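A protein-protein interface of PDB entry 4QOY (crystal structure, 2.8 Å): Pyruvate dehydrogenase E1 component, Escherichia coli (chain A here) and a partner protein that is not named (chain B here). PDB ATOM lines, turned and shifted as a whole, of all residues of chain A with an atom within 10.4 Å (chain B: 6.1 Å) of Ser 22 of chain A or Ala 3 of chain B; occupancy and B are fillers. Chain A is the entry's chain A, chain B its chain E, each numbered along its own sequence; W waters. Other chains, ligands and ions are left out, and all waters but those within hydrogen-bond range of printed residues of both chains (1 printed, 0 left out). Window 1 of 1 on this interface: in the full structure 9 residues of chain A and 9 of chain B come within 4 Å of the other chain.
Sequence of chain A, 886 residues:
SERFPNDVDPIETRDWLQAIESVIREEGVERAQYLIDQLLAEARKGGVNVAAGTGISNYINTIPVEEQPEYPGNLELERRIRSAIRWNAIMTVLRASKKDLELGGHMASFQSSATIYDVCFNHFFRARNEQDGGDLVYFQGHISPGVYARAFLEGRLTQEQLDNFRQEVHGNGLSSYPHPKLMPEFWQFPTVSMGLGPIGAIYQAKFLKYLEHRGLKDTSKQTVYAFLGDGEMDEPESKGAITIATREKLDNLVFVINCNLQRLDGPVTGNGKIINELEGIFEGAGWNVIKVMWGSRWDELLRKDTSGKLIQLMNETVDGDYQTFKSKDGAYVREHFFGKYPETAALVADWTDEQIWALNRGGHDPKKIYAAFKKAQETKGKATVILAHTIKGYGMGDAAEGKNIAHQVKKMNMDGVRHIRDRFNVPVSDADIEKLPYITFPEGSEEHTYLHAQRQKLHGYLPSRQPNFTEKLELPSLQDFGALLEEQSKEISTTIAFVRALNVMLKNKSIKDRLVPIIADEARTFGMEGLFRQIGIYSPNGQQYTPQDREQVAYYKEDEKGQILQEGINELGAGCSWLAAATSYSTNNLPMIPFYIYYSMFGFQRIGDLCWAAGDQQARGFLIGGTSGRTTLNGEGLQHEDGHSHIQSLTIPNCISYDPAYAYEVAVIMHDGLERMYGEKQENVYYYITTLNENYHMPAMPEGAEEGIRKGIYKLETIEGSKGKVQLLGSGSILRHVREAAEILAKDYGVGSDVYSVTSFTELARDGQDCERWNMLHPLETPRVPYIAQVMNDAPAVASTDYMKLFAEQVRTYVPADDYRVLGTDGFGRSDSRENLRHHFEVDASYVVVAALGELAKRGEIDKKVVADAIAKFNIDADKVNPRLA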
ATOM      1  N   ARG A  14      10.713  15.480 -20.526  1.00  0.00           N
ATOM      2  CA  ARG A  14      11.720  15.484 -19.449  1.00  0.00           C
ATOM      3  C   ARG A  14      11.078  15.057 -18.134  1.00  0.00           C
ATOM      4  O   ARG A  14      11.646  14.222 -17.444  1.00  0.00           O
ATOM      5  CB  ARG A  14      12.413  16.866 -19.265  1.00  0.00           C
ATOM      6  CG  ARG A  14      13.235  17.395 -20.454  1.00  0.00           C
ATOM      7  CD  ARG A  14      14.605  16.749 -20.646  1.00  0.00           C
ATOM      8  NE  ARG A  14      15.000  16.719 -22.059  1.00  0.00           N
ATOM      9  CZ  ARG A  14      14.918  15.646 -22.842  1.00  0.00           C
ATOM     10  NH1 ARG A  14      14.484  14.488 -22.353  1.00  0.00           N
ATOM     11  NH2 ARG A  14      15.281  15.718 -24.116  1.00  0.00           N
ATOM     12  N   ASP A  15       9.882  15.598 -17.810  1.00  0.00           N
ATOM     13  CA  ASP A  15       9.126  15.304 -16.587  1.00  0.00           C
ATOM     14  C   ASP A  15       8.720  13.835 -16.499  1.00  0.00           C
ATOM     15  O   ASP A  15       8.849  13.215 -15.442  1.00  0.00           O
ATOM     16  CB  ASP A  15       7.870  16.189 -16.519  1.00  0.00           C
ATOM     17  CG  ASP A  15       8.142  17.674 -16.408  1.00  0.00           C
ATOM     18  OD1 ASP A  15       9.327  18.075 -16.518  1.00  0.00           O
ATOM     19  OD2 ASP A  15       7.171  18.441 -16.225  1.00  0.00           O
ATOM     20  N   TRP A  16       8.248  13.281 -17.619  1.00  0.00           N
ATOM     21  CA  TRP A  16       7.794  11.895 -17.700  1.00  0.00           C
ATOM     22  C   TRP A  16       8.949  10.910 -17.551  1.00  0.00           C
ATOM     23  O   TRP A  16       8.837   9.959 -16.773  1.00  0.00           O
ATOM     24  CB  TRP A  16       7.048  11.643 -19.011  1.00  0.00           C
ATOM     25  CG  TRP A  16       5.604  12.046 -18.957  1.00  0.00           C
ATOM     26  CD1 TRP A  16       5.074  13.236 -19.355  1.00  0.00           C
ATOM     27  CD2 TRP A  16       4.505  11.261 -18.461  1.00  0.00           C
ATOM     28  NE1 TRP A  16       3.713  13.242 -19.152  1.00  0.00           N
ATOM     29  CE2 TRP A  16       3.336  12.042 -18.603  1.00  0.00           C
ATOM     30  CE3 TRP A  16       4.391   9.964 -17.915  1.00  0.00           C
ATOM     31  CZ2 TRP A  16       2.070  11.575 -18.216  1.00  0.00           C
ATOM     32  CZ3 TRP A  16       3.137   9.501 -17.538  1.00  0.00           C
ATOM     33  CH2 TRP A  16       1.996  10.301 -17.687  1.00  0.00           C
ATOM     34  N   LEU A  17      10.062  11.157 -18.280  1.00  0.00           N
ATOM     35  CA  LEU A  17      11.286  10.352 -18.255  1.00  0.00           C
ATOM     36  C   LEU A  17      12.028  10.519 -16.913  1.00  0.00           C
ATOM     37  O   LEU A  17      12.683   9.574 -16.478  1.00  0.00           O
ATOM     38  CB  LEU A  17      12.200  10.709 -19.437  1.00  0.00           C
ATOM     39  CG  LEU A  17      12.091   9.835 -20.686  1.00  0.00           C
ATOM     40  CD1 LEU A  17      10.811  10.110 -21.442  1.00  0.00           C
ATOM     41  CD2 LEU A  17      13.267  10.072 -21.610  1.00  0.00           C
ATOM     42  N   GLN A  18      11.893  11.690 -16.240  1.00  0.00           N
ATOM     43  CA  GLN A  18      12.500  11.926 -14.920  1.00  0.00           C
ATOM     44  C   GLN A  18      11.651  11.262 -13.813  1.00  0.00           C
ATOM     45  O   GLN A  18      12.175  11.006 -12.724  1.00  0.00           O
ATOM     46  CB  GLN A  18      12.690  13.430 -14.631  1.00  0.00           C
ATOM     47  CG  GLN A  18      14.042  14.002 -15.069  1.00  0.00           C
ATOM     48  CD  GLN A  18      14.059  15.522 -15.162  1.00  0.00           C
ATOM     49  OE1 GLN A  18      13.228  16.234 -14.570  1.00  0.00           O
ATOM     50  NE2 GLN A  18      15.023  16.063 -15.907  1.00  0.00           N
ATOM     51  N   ALA A  19      10.355  10.971 -14.101  1.00  0.00           N
ATOM     52  CA  ALA A  19       9.432  10.322 -13.167  1.00  0.00           C
ATOM     53  C   ALA A  19       9.701   8.802 -13.056  1.00  0.00           C
ATOM     54  O   ALA A  19       9.671   8.285 -11.939  1.00  0.00           O
ATOM     55  CB  ALA A  19       7.992  10.578 -13.575  1.00  0.00           C
ATOM     56  N   ILE A  20       9.972   8.095 -14.195  1.00  0.00           N
ATOM     57  CA  ILE A  20      10.276   6.646 -14.211  1.00  0.00           C
ATOM     58  C   ILE A  20      11.697   6.371 -13.709  1.00  0.00           C
ATOM     59  O   ILE A  20      11.928   5.301 -13.138  1.00  0.00           O
ATOM     60  CB  ILE A  20      10.054   5.910 -15.566  1.00  0.00           C
ATOM     61  CG1 ILE A  20      10.927   6.455 -16.713  1.00  0.00           C
ATOM     62  CG2 ILE A  20       8.575   5.791 -15.937  1.00  0.00           C
ATOM     63  CD1 ILE A  20      10.873   5.635 -17.925  1.00  0.00           C
ATOM     64  N   GLU A  21      12.650   7.305 -13.953  1.00  0.00           N
ATOM     65  CA  GLU A  21      14.040   7.204 -13.486  1.00  0.00           C
ATOM     66  C   GLU A  21      14.078   7.274 -11.956  1.00  0.00           C
ATOM     67  O   GLU A  21      14.841   6.544 -11.320  1.00  0.00           O
ATOM     68  CB  GLU A  21      14.895   8.330 -14.080  1.00  0.00           C
ATOM     69  CG  GLU A  21      15.460   8.041 -15.457  1.00  0.00           C
ATOM     70  CD  GLU A  21      16.209   9.216 -16.055  1.00  0.00           C
ATOM     71  OE1 GLU A  21      17.253   9.613 -15.487  1.00  0.00           O
ATOM     72  OE2 GLU A  21      15.746   9.749 -17.088  1.00  0.00           O
ATOM     73  N   SER A  22      13.231   8.158 -11.379  1.00  0.00           N
ATOM     74  CA  SER A  22      13.075   8.364  -9.942  1.00  0.00           C
ATOM     75  C   SER A  22      12.271   7.214  -9.321  1.00  0.00           C
ATOM     76  O   SER A  22      12.470   6.918  -8.147  1.00  0.00           O
ATOM     77  CB  SER A  22      12.421   9.713  -9.659  1.00  0.00           C
ATOM     78  OG  SER A  22      11.104   9.805 -10.177  1.00  0.00           O
ATOM     79  N   VAL A  23      11.392   6.550 -10.113  1.00  0.00           N
ATOM     80  CA  VAL A  23      10.614   5.372  -9.704  1.00  0.00           C
ATOM     81  C   VAL A  23      11.580   4.171  -9.564  1.00  0.00           C
ATOM     82  O   VAL A  23      11.367   3.321  -8.697  1.00  0.00           O
ATOM     83  CB  VAL A  23       9.434   5.090 -10.680  1.00  0.00           C
ATOM     84  CG1 VAL A  23       9.110   3.604 -10.782  1.00  0.00           C
ATOM     85  CG2 VAL A  23       8.196   5.866 -10.267  1.00  0.00           C
ATOM     86  N   ILE A  24      12.652   4.131 -10.393  1.00  0.00           N
ATOM     87  CA  ILE A  24      13.690   3.094 -10.365  1.00  0.00           C
ATOM     88  C   ILE A  24      14.600   3.314  -9.104  1.00  0.00           C
ATOM     89  O   ILE A  24      15.113   2.337  -8.551  1.00  0.00           O
ATOM     90  CB  ILE A  24      14.431   3.011 -11.733  1.00  0.00           C
ATOM     91  CG1 ILE A  24      13.507   2.300 -12.764  1.00  0.00           C
ATOM     92  CG2 ILE A  24      15.791   2.293 -11.633  1.00  0.00           C
ATOM     93  CD1 ILE A  24      13.840   2.462 -14.250  1.00  0.00           C
ATOM     94  N   ARG A  25      14.686   4.571  -8.595  1.00  0.00           N
ATOM     95  CA  ARG A  25      15.381   4.961  -7.350  1.00  0.00           C
ATOM     96  C   ARG A  25      14.433   4.808  -6.121  1.00  0.00           C
ATOM     97  O   ARG A  25      14.736   5.293  -5.027  1.00  0.00           O
ATOM     98  CB  ARG A  25      15.868   6.417  -7.440  1.00  0.00           C
ATOM     99  CG  ARG A  25      17.023   6.678  -8.385  1.00  0.00           C
ATOM    100  CD  ARG A  25      17.195   8.176  -8.508  1.00  0.00           C
ATOM    101  NE  ARG A  25      18.549   8.558  -8.902  1.00  0.00           N
ATOM    102  CZ  ARG A  25      19.006   9.807  -8.888  1.00  0.00           C
ATOM    103  NH1 ARG A  25      18.222  10.805  -8.494  1.00  0.00           N
ATOM    104  NH2 ARG A  25      20.250  10.068  -9.261  1.00  0.00           N
ATOM    105  N   GLU A  26      13.262   4.175  -6.344  1.00  0.00           N
ATOM    106  CA  GLU A  26      12.182   3.880  -5.392  1.00  0.00           C
ATOM    107  C   GLU A  26      11.873   2.375  -5.553  1.00  0.00           C
ATOM    108  O   GLU A  26      10.754   1.975  -5.897  1.00  0.00           O
ATOM    109  CB  GLU A  26      10.967   4.807  -5.687  1.00  0.00           C
ATOM    110  CG  GLU A  26       9.766   4.699  -4.755  1.00  0.00           C
ATOM    111  CD  GLU A  26       8.861   3.522  -5.063  1.00  0.00           C
ATOM    112  OE1 GLU A  26       8.850   3.060  -6.228  1.00  0.00           O
ATOM    113  OE2 GLU A  26       8.148   3.073  -4.137  1.00  0.00           O
ATOM    114  N   GLU A  27      12.924   1.547  -5.364  1.00  0.00           N
ATOM    115  CA  GLU A  27      12.911   0.086  -5.526  1.00  0.00           C
ATOM    116  C   GLU A  27      12.181  -0.280  -6.840  1.00  0.00           C
ATOM    117  O   GLU A  27      11.183  -1.011  -6.844  1.00  0.00           O
ATOM    118  CB  GLU A  27      12.306  -0.628  -4.292  1.00  0.00           C
ATOM    119  CG  GLU A  27      13.041  -0.400  -2.974  1.00  0.00           C
ATOM    120  CD  GLU A  27      14.559  -0.366  -2.996  1.00  0.00           C
ATOM    121  OE1 GLU A  27      15.177  -1.366  -3.428  1.00  0.00           O
ATOM    122  OE2 GLU A  27      15.131   0.662  -2.563  1.00  0.00           O
ATOM    123  N   GLY A  28      12.680   0.289  -7.934  1.00  0.00           N
ATOM    124  CA  GLY A  28      12.119   0.126  -9.266  1.00  0.00           C
ATOM    125  C   GLY A  28      12.384  -1.214  -9.904  1.00  0.00           C
ATOM    126  O   GLY A  28      12.479  -2.230  -9.206  1.00  0.00           O
ATOM    127  N   VAL A  29      12.476  -1.217 -11.256  1.00  0.00           N
ATOM    128  CA  VAL A  29      12.667  -2.398 -12.113  1.00  0.00           C
ATOM    129  C   VAL A  29      11.387  -3.266 -12.011  1.00  0.00           C
ATOM    130  O   VAL A  29      10.747  -3.506 -13.034  1.00  0.00           O
ATOM    131  CB  VAL A  29      13.981  -3.179 -11.823  1.00  0.00           C
ATOM    132  CG1 VAL A  29      14.070  -4.467 -12.636  1.00  0.00           C
ATOM    133  CG2 VAL A  29      15.203  -2.298 -12.072  1.00  0.00           C
ATOM    134  N   ARG A  31       8.763  -2.384  -9.536  1.00  0.00           N
ATOM    135  CA  ARG A  31       7.750  -1.333  -9.336  1.00  0.00           C
ATOM    136  C   ARG A  31       7.548  -0.549 -10.620  1.00  0.00           C
ATOM    137  O   ARG A  31       6.417  -0.164 -10.922  1.00  0.00           O
ATOM    138  CB  ARG A  31       8.135  -0.360  -8.199  1.00  0.00           C
ATOM    139  CG  ARG A  31       7.146   0.781  -7.939  1.00  0.00           C
ATOM    140  CD  ARG A  31       5.732   0.354  -7.550  1.00  0.00           C
ATOM    141  NE  ARG A  31       4.840   1.482  -7.268  1.00  0.00           N
ATOM    142  CZ  ARG A  31       3.514   1.391  -7.230  1.00  0.00           C
ATOM    143  NH1 ARG A  31       2.915   0.226  -7.435  1.00  0.00           N
ATOM    144  NH2 ARG A  31       2.776   2.462  -6.970  1.00  0.00           N
ATOM    145  N   ALA A  32       8.661  -0.310 -11.367  1.00  0.00           N
ATOM    146  CA  ALA A  32       8.686   0.403 -12.646  1.00  0.00           C
ATOM    147  C   ALA A  32       7.888  -0.356 -13.707  1.00  0.00           C
ATOM    148  O   ALA A  32       7.138   0.272 -14.448  1.00  0.00           O
ATOM    149  CB  ALA A  32      10.120   0.612 -13.109  1.00  0.00           C
ATOM    150  N   LEU A  35       4.033  -0.244 -12.923  1.00  0.00           N
ATOM    151  CA  LEU A  35       3.540   1.086 -13.285  1.00  0.00           C
ATOM    152  C   LEU A  35       3.425   1.256 -14.805  1.00  0.00           C
ATOM    153  O   LEU A  35       2.453   1.854 -15.258  1.00  0.00           O
ATOM    154  CB  LEU A  35       4.423   2.192 -12.690  1.00  0.00           C
ATOM    155  CG  LEU A  35       4.232   2.463 -11.194  1.00  0.00           C
ATOM    156  CD1 LEU A  35       5.431   3.161 -10.618  1.00  0.00           C
ATOM    157  CD2 LEU A  35       2.971   3.276 -10.925  1.00  0.00           C
ATOM    158  N   VAL B   1      15.783  13.957  -7.141  1.00  0.00           N
ATOM    159  CA  VAL B   1      14.438  14.498  -6.918  1.00  0.00           C
ATOM    160  C   VAL B   1      13.385  13.486  -7.440  1.00  0.00           C
ATOM    161  O   VAL B   1      13.312  13.237  -8.648  1.00  0.00           O
ATOM    162  CB  VAL B   1      14.276  15.911  -7.549  1.00  0.00           C
ATOM    163  CG1 VAL B   1      12.850  16.427  -7.397  1.00  0.00           C
ATOM    164  CG2 VAL B   1      15.267  16.901  -6.948  1.00  0.00           C
ATOM    165  N   HIS B   2      12.582  12.908  -6.515  1.00  0.00           N
ATOM    166  CA  HIS B   2      11.569  11.889  -6.817  1.00  0.00           C
ATOM    167  C   HIS B   2      10.149  12.445  -6.658  1.00  0.00           C
ATOM    168  O   HIS B   2       9.764  12.852  -5.563  1.00  0.00           O
ATOM    169  CB  HIS B   2      11.788  10.637  -5.929  1.00  0.00           C
ATOM    170  CG  HIS B   2      10.748   9.556  -6.047  1.00  0.00           C
ATOM    171  ND1 HIS B   2      10.215   9.181  -7.269  1.00  0.00           N
ATOM    172  CD2 HIS B   2      10.229   8.756  -5.086  1.00  0.00           C
ATOM    173  CE1 HIS B   2       9.362   8.203  -7.006  1.00  0.00           C
ATOM    174  NE2 HIS B   2       9.333   7.917  -5.706  1.00  0.00           N
ATOM    175  N   ALA B   3       9.381  12.464  -7.769  1.00  0.00           N
ATOM    176  CA  ALA B   3       8.003  12.956  -7.838  1.00  0.00           C
ATOM    177  C   ALA B   3       7.236  12.271  -8.979  1.00  0.00           C
ATOM    178  O   ALA B   3       7.861  11.803  -9.938  1.00  0.00           O
ATOM    179  CB  ALA B   3       8.000  14.467  -8.043  1.00  0.00           C
ATOM    180  N   THR B   4       5.881  12.198  -8.869  1.00  0.00           N
ATOM    181  CA  THR B   4       5.016  11.610  -9.913  1.00  0.00           C
ATOM    182  C   THR B   4       4.915  12.606 -11.110  1.00  0.00           C
ATOM    183  O   THR B   4       5.120  13.807 -10.888  1.00  0.00           O
ATOM    184  CB  THR B   4       3.616  11.201  -9.366  1.00  0.00           C
ATOM    185  OG1 THR B   4       2.834  12.346  -9.028  1.00  0.00           O
ATOM    186  CG2 THR B   4       3.686  10.241  -8.202  1.00  0.00           C
ATOM    187  N   PRO B   5       4.608  12.158 -12.370  1.00  0.00           N
ATOM    188  CA  PRO B   5       4.535  13.116 -13.494  1.00  0.00           C
ATOM    189  C   PRO B   5       3.411  14.140 -13.325  1.00  0.00           C
ATOM    190  O   PRO B   5       3.422  15.165 -14.011  1.00  0.00           O
ATOM    191  CB  PRO B   5       4.320  12.226 -14.727  1.00  0.00           C
ATOM    192  CG  PRO B   5       3.761  10.979 -14.206  1.00  0.00           C
ATOM    193  CD  PRO B   5       4.336  10.784 -12.836  1.00  0.00           C
ATOM    194  N   LEU B   6       2.472  13.873 -12.387  1.00  0.00           N
ATOM    195  CA  LEU B   6       1.369  14.761 -12.030  1.00  0.00           C
ATOM    196  C   LEU B   6       1.911  15.930 -11.185  1.00  0.00           C
ATOM    197  O   LEU B   6       1.579  17.086 -11.449  1.00  0.00           O
ATOM    198  CB  LEU B   6       0.289  13.972 -11.268  1.00  0.00           C
ATOM    199  CG  LEU B   6      -0.899  14.784 -10.765  1.00  0.00           C
ATOM    200  CD1 LEU B   6      -1.665  15.386 -11.916  1.00  0.00           C
ATOM    201  CD2 LEU B   6      -1.806  13.950  -9.871  1.00  0.00           C
ATOM    202  N   ILE B   7       2.759  15.614 -10.184  1.00  0.00           N
ATOM    203  CA  ILE B   7       3.391  16.579  -9.272  1.00  0.00           C
ATOM    204  C   ILE B   7       4.466  17.392 -10.028  1.00  0.00           C
ATOM    205  O   ILE B   7       4.640  18.585  -9.750  1.00  0.00           O
ATOM    206  CB  ILE B   7       3.963  15.859  -8.005  1.00  0.00           C
ATOM    207  CG1 ILE B   7       2.885  14.995  -7.265  1.00  0.00           C
ATOM    208  CG2 ILE B   7       4.691  16.818  -7.043  1.00  0.00           C
ATOM    209  CD1 ILE B   7       1.508  15.654  -6.880  1.00  0.00           C
ATOM    210  N   ARG B   8       5.155  16.755 -10.989  1.00  0.00           N
ATOM    211  CA  ARG B   8       6.168  17.406 -11.821  1.00  0.00           C
ATOM    212  C   ARG B   8       5.514  18.441 -12.753  1.00  0.00           C
ATOM    213  O   ARG B   8       6.076  19.518 -12.945  1.00  0.00           O
ATOM    214  CB  ARG B   8       6.969  16.372 -12.626  1.00  0.00           C
ATOM    215  CG  ARG B   8       7.945  15.566 -11.783  1.00  0.00           C
ATOM    216  CD  ARG B   8       8.656  14.530 -12.618  1.00  0.00           C
ATOM    217  NE  ARG B   8       9.529  13.683 -11.808  1.00  0.00           N
ATOM    218  CZ  ARG B   8      10.804  13.951 -11.553  1.00  0.00           C
ATOM    219  NH1 ARG B   8      11.368  15.050 -12.039  1.00  0.00           N
ATOM    220  NH2 ARG B   8      11.524  13.127 -10.804  1.00  0.00           N
ATOM    221  N   LEU B  18      11.060  21.675  -7.640  1.00  0.00           N
ATOM    222  CA  LEU B  18      10.945  20.465  -6.811  1.00  0.00           C
ATOM    223  C   LEU B  18      12.274  20.064  -6.128  1.00  0.00           C
ATOM    224  O   LEU B  18      12.261  19.192  -5.257  1.00  0.00           O
ATOM    225  CB  LEU B  18      10.352  19.273  -7.596  1.00  0.00           C
ATOM    226  CG  LEU B  18       8.859  19.356  -7.993  1.00  0.00           C
ATOM    227  CD1 LEU B  18       8.466  18.198  -8.879  1.00  0.00           C
ATOM    228  CD2 LEU B  18       7.933  19.377  -6.781  1.00  0.00           C
ATOM    229  N   ARG B  29       9.136  10.523  -1.875  1.00  0.00           N
ATOM    230  CA  ARG B  29       8.434  11.097  -3.018  1.00  0.00           C
ATOM    231  C   ARG B  29       7.782  12.425  -2.641  1.00  0.00           C
ATOM    232  O   ARG B  29       7.155  12.518  -1.580  1.00  0.00           O
ATOM    233  CB  ARG B  29       7.381  10.112  -3.541  1.00  0.00           C
ATOM    234  CG  ARG B  29       6.952  10.380  -4.979  1.00  0.00           C
ATOM    235  CD  ARG B  29       6.009   9.314  -5.500  1.00  0.00           C
ATOM    236  NE  ARG B  29       4.653   9.451  -4.962  1.00  0.00           N
ATOM    237  CZ  ARG B  29       4.133   8.663  -4.025  1.00  0.00           C
ATOM    238  NH1 ARG B  29       4.847   7.669  -3.511  1.00  0.00           N
ATOM    239  NH2 ARG B  29       2.893   8.858  -3.600  1.00  0.00           N
ATOM    240  N   ILE B  30       7.930  13.455  -3.504  1.00  0.00           N
ATOM    241  CA  ILE B  30       7.304  14.757  -3.258  1.00  0.00           C
ATOM    242  C   ILE B  30       5.813  14.628  -3.636  1.00  0.00           C
ATOM    243  O   ILE B  30       5.483  14.344  -4.794  1.00  0.00           O
ATOM    244  CB  ILE B  30       8.028  15.943  -3.961  1.00  0.00           C
ATOM    245  CG1 ILE B  30       9.514  15.988  -3.560  1.00  0.00           C
ATOM    246  CG2 ILE B  30       7.340  17.277  -3.627  1.00  0.00           C
ATOM    247  CD1 ILE B  30      10.416  16.534  -4.593  1.00  0.00           C
HETATM  248  O   HOH W   1       7.414   8.968  -9.705  1.00  0.00           O
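O of Ala 19 of chain A sits at hydrogen-bond distance from OG of Ser 22 of chain A (2.7 Å).
The side-chain hydroxyl (OG) of Ser 22 of chain A is in hydrogen-bond range of the backbone carbonyl oxygen (O) of Gln 18 of chain A, at 3.0 Å.
O of Val 1 of chain B lies within hydrogen-bond range of NH2 of Arg 8 of chain B, at 2.8 Å.
The backbone carbonyl oxygen (O) of Ala 3 of chain B sits at hydrogen-bond distance from the guanidinium group (NE) of Arg 8 of chain B.
O of His 2 of chain B lies within hydrogen-bond range of N of Ile 30 of chain B, 2.8 Å away.
Among the printed residues, pairs that only touch across the chains: Asp 15 of chain A with Arg 8 of chain B, Trp 16 of chain A with Pro 5 of chain B, Ala 19 of chain A with Ala 3 of chain B, Ala 19 of chain A with Pro 5 of chain B, Ala 19 of chain A with Arg 8 of chain B, Ser 22 of chain A with Val 1 of chain B, Ser 22 of chain A with Ala 3 of chain B and Glu 26 of chain A with His 2 of chain B.
Printed residues of chain B that touch a printed residue of chain A: Val 1, His 2, Ala 3, Pro 5 and Arg 8.
Hydrophobic or aromatic side chains of chain B within 4 Å of the printed part of chain A: His 2 and Pro 5.
Of the 19 printed residues of chain A, 6 touch a printed residue of chain B.
Printed residues of chain A that touch a printed residue of chain B: Asp 15, Trp 16, Gln 18, Ala 19, Ser 22 and Glu 26.
Hydrophobic or aromatic side chains of chain A within 4 Å of the printed part of chain B: Trp 16 and Ala 19.
Among the printed residues, 11 pairs touch across the chains.
Among the printed residues, no Asp or Glu carboxylate lies within 4 Å of a Lys or Arg side-chain nitrogen of the other chain.
The side-chain hydroxyl of Ser 22 of chain A sits at hydrogen-bond distance from the guanidinium group of Arg 8 of chain B (3.4 Å).
The guanidinium group (NH2) of Arg 8 of chain B lies within hydrogen-bond range of the backbone carbonyl oxygen (O) of Gln 18 of chain A (2.9 Å).
OG of Ser 22 of chain A sits at hydrogen-bond distance from ND1 of His 2 of chain B, 3.1 Å away.
Ala 3 of chain B touches two residues of chain A.
Of the printed residues of chain A, His 2 of chain B touches Ser 22 (3.1 Å) and Glu 26 (3.4 Å).
No residue of chain A comes within 4 Å of Ile 30 of chain B.
Printed residues of chain A within 4 Å of Pro 5 of chain B: Trp 16 (3.7 Å) and Ala 19 (3.7 Å).
Printed residues of chain A within 4 Å of Arg 8 of chain B: Asp 15, Gln 18, Ala 19 and Ser 22.
Of the printed residues of chain A, Val 1 of chain B touches Ser 22 (3.8 Å).
Of the printed residues of chain B, Gln 18 of chain A touches Arg 8 (2.9 Å).
Of the printed residues of chain B, Glu 26 of chain A touches His 2.
The nearest residue of chain B that does not touch Ser 22 of chain A is Thr 4 of chain B (5.9 Å).
Water W1 lies within hydrogen-bond range of O of Ala 3 of chain B (2.9 Å) and O of Ala 19 of chain A (3.2 Å).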
